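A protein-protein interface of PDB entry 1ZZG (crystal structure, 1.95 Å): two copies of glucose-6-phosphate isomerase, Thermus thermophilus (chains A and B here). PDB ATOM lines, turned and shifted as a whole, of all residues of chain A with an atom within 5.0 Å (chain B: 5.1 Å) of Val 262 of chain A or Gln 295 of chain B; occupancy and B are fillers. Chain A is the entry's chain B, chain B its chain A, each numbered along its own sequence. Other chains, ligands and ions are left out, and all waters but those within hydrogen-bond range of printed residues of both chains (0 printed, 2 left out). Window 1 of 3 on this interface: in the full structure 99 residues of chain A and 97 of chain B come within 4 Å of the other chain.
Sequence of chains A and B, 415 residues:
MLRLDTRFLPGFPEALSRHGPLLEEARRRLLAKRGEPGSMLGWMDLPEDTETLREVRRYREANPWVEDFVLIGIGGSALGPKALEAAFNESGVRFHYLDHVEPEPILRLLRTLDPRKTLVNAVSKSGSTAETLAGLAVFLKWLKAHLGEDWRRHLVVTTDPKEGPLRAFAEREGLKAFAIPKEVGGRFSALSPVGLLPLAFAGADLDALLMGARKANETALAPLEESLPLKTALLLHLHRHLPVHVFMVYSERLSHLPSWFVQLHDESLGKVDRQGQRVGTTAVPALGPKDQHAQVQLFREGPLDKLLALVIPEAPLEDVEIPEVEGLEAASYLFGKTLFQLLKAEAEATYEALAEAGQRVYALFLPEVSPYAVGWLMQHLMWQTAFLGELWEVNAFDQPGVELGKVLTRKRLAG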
ATOM      1  N   PRO A 258      33.493 -34.133  21.298  1.00  0.00           N
ATOM      2  CA  PRO A 258      32.648 -32.956  21.055  1.00  0.00           C
ATOM      3  C   PRO A 258      31.616 -32.707  22.151  1.00  0.00           C
ATOM      4  O   PRO A 258      31.424 -31.570  22.578  1.00  0.00           O
ATOM      5  CB  PRO A 258      32.009 -33.263  19.706  1.00  0.00           C
ATOM      6  CG  PRO A 258      33.102 -34.024  19.002  1.00  0.00           C
ATOM      7  CD  PRO A 258      33.567 -34.978  20.089  1.00  0.00           C
ATOM      8  N   SER A 259      30.955 -33.770  22.605  1.00  0.00           N
ATOM      9  CA  SER A 259      29.949 -33.651  23.659  1.00  0.00           C
ATOM     10  C   SER A 259      30.568 -33.097  24.937  1.00  0.00           C
ATOM     11  O   SER A 259      29.965 -32.275  25.625  1.00  0.00           O
ATOM     12  CB  SER A 259      29.330 -35.015  23.960  1.00  0.00           C
ATOM     13  OG  SER A 259      28.522 -35.446  22.889  1.00  0.00           O
ATOM     14  N   TRP A 260      31.770 -33.562  25.257  1.00  0.00           N
ATOM     15  CA  TRP A 260      32.459 -33.088  26.450  1.00  0.00           C
ATOM     16  C   TRP A 260      32.701 -31.587  26.317  1.00  0.00           C
ATOM     17  O   TRP A 260      32.435 -30.826  27.249  1.00  0.00           O
ATOM     18  CB  TRP A 260      33.794 -33.814  26.620  1.00  0.00           C
ATOM     19  CG  TRP A 260      34.667 -33.204  27.673  1.00  0.00           C
ATOM     20  CD1 TRP A 260      34.583 -33.391  29.022  1.00  0.00           C
ATOM     21  CD2 TRP A 260      35.738 -32.280  27.459  1.00  0.00           C
ATOM     22  NE1 TRP A 260      35.538 -32.641  29.662  1.00  0.00           N
ATOM     23  CE2 TRP A 260      36.264 -31.951  28.726  1.00  0.00           C
ATOM     24  CE3 TRP A 260      36.309 -31.701  26.315  1.00  0.00           C
ATOM     25  CZ2 TRP A 260      37.333 -31.064  28.886  1.00  0.00           C
ATOM     26  CZ3 TRP A 260      37.377 -30.817  26.475  1.00  0.00           C
ATOM     27  CH2 TRP A 260      37.878 -30.511  27.755  1.00  0.00           C
ATOM     28  N   PHE A 261      33.197 -31.158  25.159  1.00  0.00           N
ATOM     29  CA  PHE A 261      33.449 -29.732  24.954  1.00  0.00           C
ATOM     30  C   PHE A 261      32.174 -28.893  25.009  1.00  0.00           C
ATOM     31  O   PHE A 261      32.178 -27.777  25.536  1.00  0.00           O
ATOM     32  CB  PHE A 261      34.128 -29.465  23.619  1.00  0.00           C
ATOM     33  CG  PHE A 261      34.251 -28.003  23.311  1.00  0.00           C
ATOM     34  CD1 PHE A 261      35.161 -27.209  24.003  1.00  0.00           C
ATOM     35  CD2 PHE A 261      33.408 -27.402  22.383  1.00  0.00           C
ATOM     36  CE1 PHE A 261      35.227 -25.836  23.777  1.00  0.00           C
ATOM     37  CE2 PHE A 261      33.464 -26.028  22.147  1.00  0.00           C
ATOM     38  CZ  PHE A 261      34.373 -25.243  22.846  1.00  0.00           C
ATOM     39  N   VAL A 262      31.089 -29.418  24.447  1.00  0.00           N
ATOM     40  CA  VAL A 262      29.819 -28.699  24.453  1.00  0.00           C
ATOM     41  C   VAL A 262      29.413 -28.381  25.886  1.00  0.00           C
ATOM     42  O   VAL A 262      28.975 -27.263  26.173  1.00  0.00           O
ATOM     43  CB  VAL A 262      28.691 -29.516  23.763  1.00  0.00           C
ATOM     44  CG1 VAL A 262      27.330 -28.859  24.011  1.00  0.00           C
ATOM     45  CG2 VAL A 262      28.952 -29.588  22.260  1.00  0.00           C
ATOM     46  N   GLN A 263      29.557 -29.352  26.787  1.00  0.00           N
ATOM     47  CA  GLN A 263      29.207 -29.114  28.185  1.00  0.00           C
ATOM     48  C   GLN A 263      30.146 -28.075  28.780  1.00  0.00           C
ATOM     49  O   GLN A 263      29.709 -27.160  29.478  1.00  0.00           O
ATOM     50  CB  GLN A 263      29.318 -30.380  29.035  1.00  0.00           C
ATOM     51  CG  GLN A 263      29.149 -30.064  30.527  1.00  0.00           C
ATOM     52  CD  GLN A 263      29.644 -31.159  31.451  1.00  0.00           C
ATOM     53  OE1 GLN A 263      30.678 -31.779  31.201  1.00  0.00           O
ATOM     54  NE2 GLN A 263      28.917 -31.383  32.542  1.00  0.00           N
ATOM     55  N   LEU A 264      31.439 -28.233  28.519  1.00  0.00           N
ATOM     56  CA  LEU A 264      32.440 -27.305  29.036  1.00  0.00           C
ATOM     57  C   LEU A 264      32.101 -25.864  28.648  1.00  0.00           C
ATOM     58  O   LEU A 264      32.019 -24.976  29.496  1.00  0.00           O
ATOM     59  CB  LEU A 264      33.830 -27.668  28.497  1.00  0.00           C
ATOM     60  CG  LEU A 264      34.965 -26.743  28.949  1.00  0.00           C
ATOM     61  CD1 LEU A 264      35.102 -26.819  30.460  1.00  0.00           C
ATOM     62  CD2 LEU A 264      36.270 -27.120  28.264  1.00  0.00           C
ATOM     63  N   HIS A 265      31.901 -25.651  27.353  1.00  0.00           N
ATOM     64  CA  HIS A 265      31.587 -24.335  26.808  1.00  0.00           C
ATOM     65  C   HIS A 265      30.219 -23.782  27.221  1.00  0.00           C
ATOM     66  O   HIS A 265      30.125 -22.667  27.729  1.00  0.00           O
ATOM     67  CB  HIS A 265      31.665 -24.387  25.284  1.00  0.00           C
ATOM     68  CG  HIS A 265      31.443 -23.065  24.627  1.00  0.00           C
ATOM     69  ND1 HIS A 265      32.456 -22.153  24.431  1.00  0.00           N
ATOM     70  CD2 HIS A 265      30.315 -22.487  24.149  1.00  0.00           C
ATOM     71  CE1 HIS A 265      31.963 -21.069  23.856  1.00  0.00           C
ATOM     72  NE2 HIS A 265      30.667 -21.247  23.674  1.00  0.00           N
ATOM     73  N   ASP A 266      29.169 -24.565  26.982  1.00  0.00           N
ATOM     74  CA  ASP A 266      27.794 -24.179  27.306  1.00  0.00           C
ATOM     75  C   ASP A 266      27.560 -23.873  28.785  1.00  0.00           C
ATOM     76  O   ASP A 266      27.098 -22.794  29.141  1.00  0.00           O
ATOM     77  CB  ASP A 266      26.824 -25.292  26.896  1.00  0.00           C
ATOM     78  CG  ASP A 266      26.413 -25.220  25.439  1.00  0.00           C
ATOM     79  OD1 ASP A 266      27.106 -24.561  24.634  1.00  0.00           O
ATOM     80  OD2 ASP A 266      25.389 -25.847  25.098  1.00  0.00           O
ATOM     81  N   GLU A 267      27.879 -24.836  29.641  1.00  0.00           N
ATOM     82  CA  GLU A 267      27.661 -24.679  31.070  1.00  0.00           C
ATOM     83  C   GLU A 267      28.565 -23.637  31.722  1.00  0.00           C
ATOM     84  O   GLU A 267      28.180 -23.014  32.707  1.00  0.00           O
ATOM     85  CB  GLU A 267      27.833 -26.036  31.761  1.00  0.00           C
ATOM     86  CG  GLU A 267      26.887 -26.276  32.917  1.00  0.00           C
ATOM     87  CD  GLU A 267      26.953 -27.702  33.429  1.00  0.00           C
ATOM     88  OE1 GLU A 267      28.054 -28.139  33.821  1.00  0.00           O
ATOM     89  OE2 GLU A 267      25.904 -28.385  33.437  1.00  0.00           O
ATOM     90  N   ALA A 283      27.507 -23.964  21.525  1.00  0.00           N
ATOM     91  CA  ALA A 283      28.477 -24.922  20.996  1.00  0.00           C
ATOM     92  C   ALA A 283      27.716 -26.052  20.296  1.00  0.00           C
ATOM     93  O   ALA A 283      26.748 -26.584  20.838  1.00  0.00           O
ATOM     94  CB  ALA A 283      29.342 -25.493  22.120  1.00  0.00           C
ATOM     95  N   VAL A 284      28.165 -26.407  19.096  1.00  0.00           N
ATOM     96  CA  VAL A 284      27.524 -27.447  18.299  1.00  0.00           C
ATOM     97  C   VAL A 284      28.542 -28.546  17.978  1.00  0.00           C
ATOM     98  O   VAL A 284      29.590 -28.290  17.387  1.00  0.00           O
ATOM     99  CB  VAL A 284      26.944 -26.832  17.004  1.00  0.00           C
ATOM    100  CG1 VAL A 284      26.359 -27.916  16.098  1.00  0.00           C
ATOM    101  CG2 VAL A 284      25.870 -25.815  17.374  1.00  0.00           C
ATOM    102  N   PRO A 285      28.237 -29.791  18.369  1.00  0.00           N
ATOM    103  CA  PRO A 285      29.131 -30.925  18.133  1.00  0.00           C
ATOM    104  C   PRO A 285      29.103 -31.492  16.716  1.00  0.00           C
ATOM    105  O   PRO A 285      28.046 -31.619  16.110  1.00  0.00           O
ATOM    106  CB  PRO A 285      28.663 -31.936  19.177  1.00  0.00           C
ATOM    107  CG  PRO A 285      27.193 -31.734  19.166  1.00  0.00           C
ATOM    108  CD  PRO A 285      27.040 -30.215  19.122  1.00  0.00           C
ATOM    109  N   VAL B 284      20.443 -28.330  16.982  1.00  0.00           N
ATOM    110  CA  VAL B 284      21.363 -28.729  18.044  1.00  0.00           C
ATOM    111  C   VAL B 284      20.770 -29.927  18.777  1.00  0.00           C
ATOM    112  O   VAL B 284      19.683 -29.840  19.346  1.00  0.00           O
ATOM    113  CB  VAL B 284      21.581 -27.569  19.048  1.00  0.00           C
ATOM    114  CG1 VAL B 284      22.527 -28.002  20.155  1.00  0.00           C
ATOM    115  CG2 VAL B 284      22.139 -26.358  18.326  1.00  0.00           C
ATOM    116  N   PRO B 285      21.483 -31.068  18.774  1.00  0.00           N
ATOM    117  CA  PRO B 285      21.005 -32.286  19.440  1.00  0.00           C
ATOM    118  C   PRO B 285      21.160 -32.248  20.963  1.00  0.00           C
ATOM    119  O   PRO B 285      22.120 -31.684  21.484  1.00  0.00           O
ATOM    120  CB  PRO B 285      21.866 -33.374  18.805  1.00  0.00           C
ATOM    121  CG  PRO B 285      23.200 -32.664  18.654  1.00  0.00           C
ATOM    122  CD  PRO B 285      22.798 -31.287  18.139  1.00  0.00           C
ATOM    123  N   ALA B 286      20.205 -32.851  21.666  1.00  0.00           N
ATOM    124  CA  ALA B 286      20.247 -32.916  23.121  1.00  0.00           C
ATOM    125  C   ALA B 286      19.491 -34.143  23.594  1.00  0.00           C
ATOM    126  O   ALA B 286      18.584 -34.634  22.915  1.00  0.00           O
ATOM    127  CB  ALA B 286      19.639 -31.664  23.730  1.00  0.00           C
ATOM    128  N   ASP B 291      21.438 -33.889  29.424  1.00  0.00           N
ATOM    129  CA  ASP B 291      21.767 -32.531  29.017  1.00  0.00           C
ATOM    130  C   ASP B 291      21.294 -31.437  29.975  1.00  0.00           C
ATOM    131  O   ASP B 291      21.505 -30.248  29.730  1.00  0.00           O
ATOM    132  CB  ASP B 291      21.301 -32.276  27.585  1.00  0.00           C
ATOM    133  CG  ASP B 291      22.335 -32.735  26.571  1.00  0.00           C
ATOM    134  OD1 ASP B 291      23.512 -32.342  26.736  1.00  0.00           O
ATOM    135  OD2 ASP B 291      21.993 -33.478  25.628  1.00  0.00           O
ATOM    136  N   GLN B 292      20.668 -31.842  31.076  1.00  0.00           N
ATOM    137  CA  GLN B 292      20.248 -30.890  32.099  1.00  0.00           C
ATOM    138  C   GLN B 292      21.561 -30.605  32.829  1.00  0.00           C
ATOM    139  O   GLN B 292      21.686 -29.639  33.587  1.00  0.00           O
ATOM    140  CB  GLN B 292      19.246 -31.529  33.070  1.00  0.00           C
ATOM    141  CG  GLN B 292      17.929 -31.978  32.436  1.00  0.00           C
ATOM    142  CD  GLN B 292      17.053 -32.798  33.381  1.00  0.00           C
ATOM    143  OE1 GLN B 292      16.019 -33.332  32.975  1.00  0.00           O
ATOM    144  NE2 GLN B 292      17.467 -32.903  34.643  1.00  0.00           N
ATOM    145  N   HIS B 293      22.543 -31.466  32.563  1.00  0.00           N
ATOM    146  CA  HIS B 293      23.866 -31.383  33.164  1.00  0.00           C
ATOM    147  C   HIS B 293      24.912 -31.020  32.112  1.00  0.00           C
ATOM    148  O   HIS B 293      26.058 -31.473  32.202  1.00  0.00           O
ATOM    149  CB  HIS B 293      24.258 -32.736  33.777  1.00  0.00           C
ATOM    150  CG  HIS B 293      23.262 -33.284  34.751  1.00  0.00           C
ATOM    151  ND1 HIS B 293      23.369 -33.098  36.112  1.00  0.00           N
ATOM    152  CD2 HIS B 293      22.146 -34.028  34.560  1.00  0.00           C
ATOM    153  CE1 HIS B 293      22.365 -33.706  36.719  1.00  0.00           C
ATOM    154  NE2 HIS B 293      21.608 -34.278  35.800  1.00  0.00           N
ATOM    155  N   ALA B 294      24.532 -30.228  31.109  1.00  0.00           N
ATOM    156  CA  ALA B 294      25.491 -29.851  30.076  1.00  0.00           C
ATOM    157  C   ALA B 294      25.064 -28.676  29.202  1.00  0.00           C
ATOM    158  O   ALA B 294      25.828 -27.729  29.015  1.00  0.00           O
ATOM    159  CB  ALA B 294      25.811 -31.061  29.192  1.00  0.00           C
ATOM    160  N   GLN B 295      23.855 -28.729  28.656  1.00  0.00           N
ATOM    161  CA  GLN B 295      23.402 -27.645  27.793  1.00  0.00           C
ATOM    162  C   GLN B 295      22.290 -26.782  28.379  1.00  0.00           C
ATOM    163  O   GLN B 295      22.150 -25.614  28.008  1.00  0.00           O
ATOM    164  CB  GLN B 295      22.950 -28.206  26.444  1.00  0.00           C
ATOM    165  CG  GLN B 295      24.019 -29.002  25.718  1.00  0.00           C
ATOM    166  CD  GLN B 295      23.567 -29.455  24.341  1.00  0.00           C
ATOM    167  OE1 GLN B 295      23.479 -28.657  23.405  1.00  0.00           O
ATOM    168  NE2 GLN B 295      23.274 -30.741  24.212  1.00  0.00           N
ATOM    169  N   VAL B 296      21.504 -27.351  29.286  1.00  0.00           N
ATOM    170  CA  VAL B 296      20.398 -26.625  29.895  1.00  0.00           C
ATOM    171  C   VAL B 296      20.833 -25.336  30.581  1.00  0.00           C
ATOM    172  O   VAL B 296      20.086 -24.357  30.588  1.00  0.00           O
ATOM    173  CB  VAL B 296      19.637 -27.518  30.898  1.00  0.00           C
ATOM    174  CG1 VAL B 296      18.664 -26.678  31.720  1.00  0.00           C
ATOM    175  CG2 VAL B 296      18.869 -28.594  30.140  1.00  0.00           C
ATOM    176  N   GLN B 297      22.034 -25.331  31.160  1.00  0.00           N
ATOM    177  CA  GLN B 297      22.539 -24.133  31.827  1.00  0.00           C
ATOM    178  C   GLN B 297      22.536 -22.981  30.825  1.00  0.00           C
ATOM    179  O   GLN B 297      22.088 -21.877  31.136  1.00  0.00           O
ATOM    180  CB  GLN B 297      23.956 -24.380  32.370  1.00  0.00           C
ATOM    181  CG  GLN B 297      24.722 -23.131  32.804  1.00  0.00           C
ATOM    182  CD  GLN B 297      23.969 -22.266  33.807  1.00  0.00           C
ATOM    183  OE1 GLN B 297      23.415 -22.767  34.793  1.00  0.00           O
ATOM    184  NE2 GLN B 297      23.962 -20.956  33.567  1.00  0.00           N
ATOM    185  N   LEU B 298      23.016 -23.245  29.616  1.00  0.00           N
ATOM    186  CA  LEU B 298      23.038 -22.221  28.580  1.00  0.00           C
ATOM    187  C   LEU B 298      21.614 -21.826  28.180  1.00  0.00           C
ATOM    188  O   LEU B 298      21.334 -20.649  27.957  1.00  0.00           O
ATOM    189  CB  LEU B 298      23.788 -22.713  27.341  1.00  0.00           C
ATOM    190  CG  LEU B 298      23.586 -21.868  26.074  1.00  0.00           C
ATOM    191  CD1 LEU B 298      24.369 -20.568  26.192  1.00  0.00           C
ATOM    192  CD2 LEU B 298      24.052 -22.642  24.853  1.00  0.00           C
ATOM    193  N   PHE B 299      20.715 -22.802  28.082  1.00  0.00           N
ATOM    194  CA  PHE B 299      19.342 -22.497  27.697  1.00  0.00           C
ATOM    195  C   PHE B 299      18.655 -21.650  28.768  1.00  0.00           C
ATOM    196  O   PHE B 299      17.807 -20.814  28.461  1.00  0.00           O
ATOM    197  CB  PHE B 299      18.525 -23.782  27.472  1.00  0.00           C
ATOM    198  CG  PHE B 299      19.144 -24.748  26.484  1.00  0.00           C
ATOM    199  CD1 PHE B 299      19.992 -24.301  25.475  1.00  0.00           C
ATOM    200  CD2 PHE B 299      18.864 -26.110  26.568  1.00  0.00           C
ATOM    201  CE1 PHE B 299      20.560 -25.197  24.563  1.00  0.00           C
ATOM    202  CE2 PHE B 299      19.423 -27.016  25.662  1.00  0.00           C
ATOM    203  CZ  PHE B 299      20.272 -26.558  24.658  1.00  0.00           C
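The side-chain amide nitrogen of Gln 263 of chain A sits at hydrogen-bond distance from the backbone carbonyl oxygen of His 293 of chain B, at 2.9 Å.
The side-chain carboxylate of Glu 267 of chain A lies close to the backbone carbonyl oxygen of His 293 of chain B, at 3.3 Å.
The backbone NH (N) of Ala 294 of chain B is in hydrogen-bond range of the side-chain carboxylate (OE2) of Glu 267 of chain A, at 3.3 Å.
N of Ala 283 of chain A sits at hydrogen-bond distance from OD1 of Asp 266 of chain A (3.2 Å).
The backbone carbonyl oxygen (O) of Pro 285 of chain B sits at hydrogen-bond distance from the side-chain amide nitrogen (NE2) of Gln 295 of chain B (3.1 Å).
The side-chain amide nitrogen of Gln 295 of chain B sits at hydrogen-bond distance from the side-chain carboxylate of Asp 291 of chain B, 3.0 Å away.
Of the 12 printed residues of chain B, 6 touch a printed residue of chain A.
Along chain B the printed residues that touch a printed residue of chain A span positions 284 to 298.
Of the 13 printed residues of chain A, 5 touch a printed residue of chain B.
Hydrophobic or aromatic side chains of chain A that line the printed part of chain B: Val 262 and Val 284.
Along chain A the printed residues that touch a printed residue of chain B span positions 262 to 284.
Of chain B, only Gln 295 comes within 4 Å of Val 262 of chain A.
Gln 295 of chain B touches two residues of chain A.
Printed residues of chain A within 4 Å of Ala 294 of chain B: Gln 263, Asp 266 and Glu 267.
Of the printed residues of chain B, Glu 267 of chain A touches His 293, Ala 294 and Gln 297.
Printed residues of chain A within 4 Å of Val 284 of chain B: Val 284.
Of the printed residues of chain A, Leu 298 of chain B touches Asp 266.
Pro 258 of chain A touches none of the printed residues of chain B.
The nearest residue of chain A that does not touch Gln 295 of chain B is Ala 283 of chain A (4.6 Å).
The nearest printed residue of chain A that does not touch Leu 298 of chain B is Ala 283 of chain A (5.0 Å).
Val 262 of chain A touches Gln 295 of chain B.
CB of Gln 263 of chain A touches CB of Ala 294 of chain B, at 3.6 Å.
Ala 294 of chain B touches Asp 266 of chain A (O to CB, 3.4 Å).
Gln 295 of chain B touches Asp 266 of chain A (CG to OD2, 3.5 Å).
Asp 266 of chain A touches Leu 298 of chain B.
Glu 267 of chain A touches Gln 297 of chain B (O to CG, 3.5 Å).
CG2 of Val 284 of chain B touches CG2 of Val 284 of chain A (3.9 Å).
Val 284 of chain A touches its own counterpart, Val 284 of chain B.
Positions printed for both chains: 284 and 285.
Of the 10 pairs that touch across the chains among the printed residues, 1 has its exchanged pair printed and touching as well.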
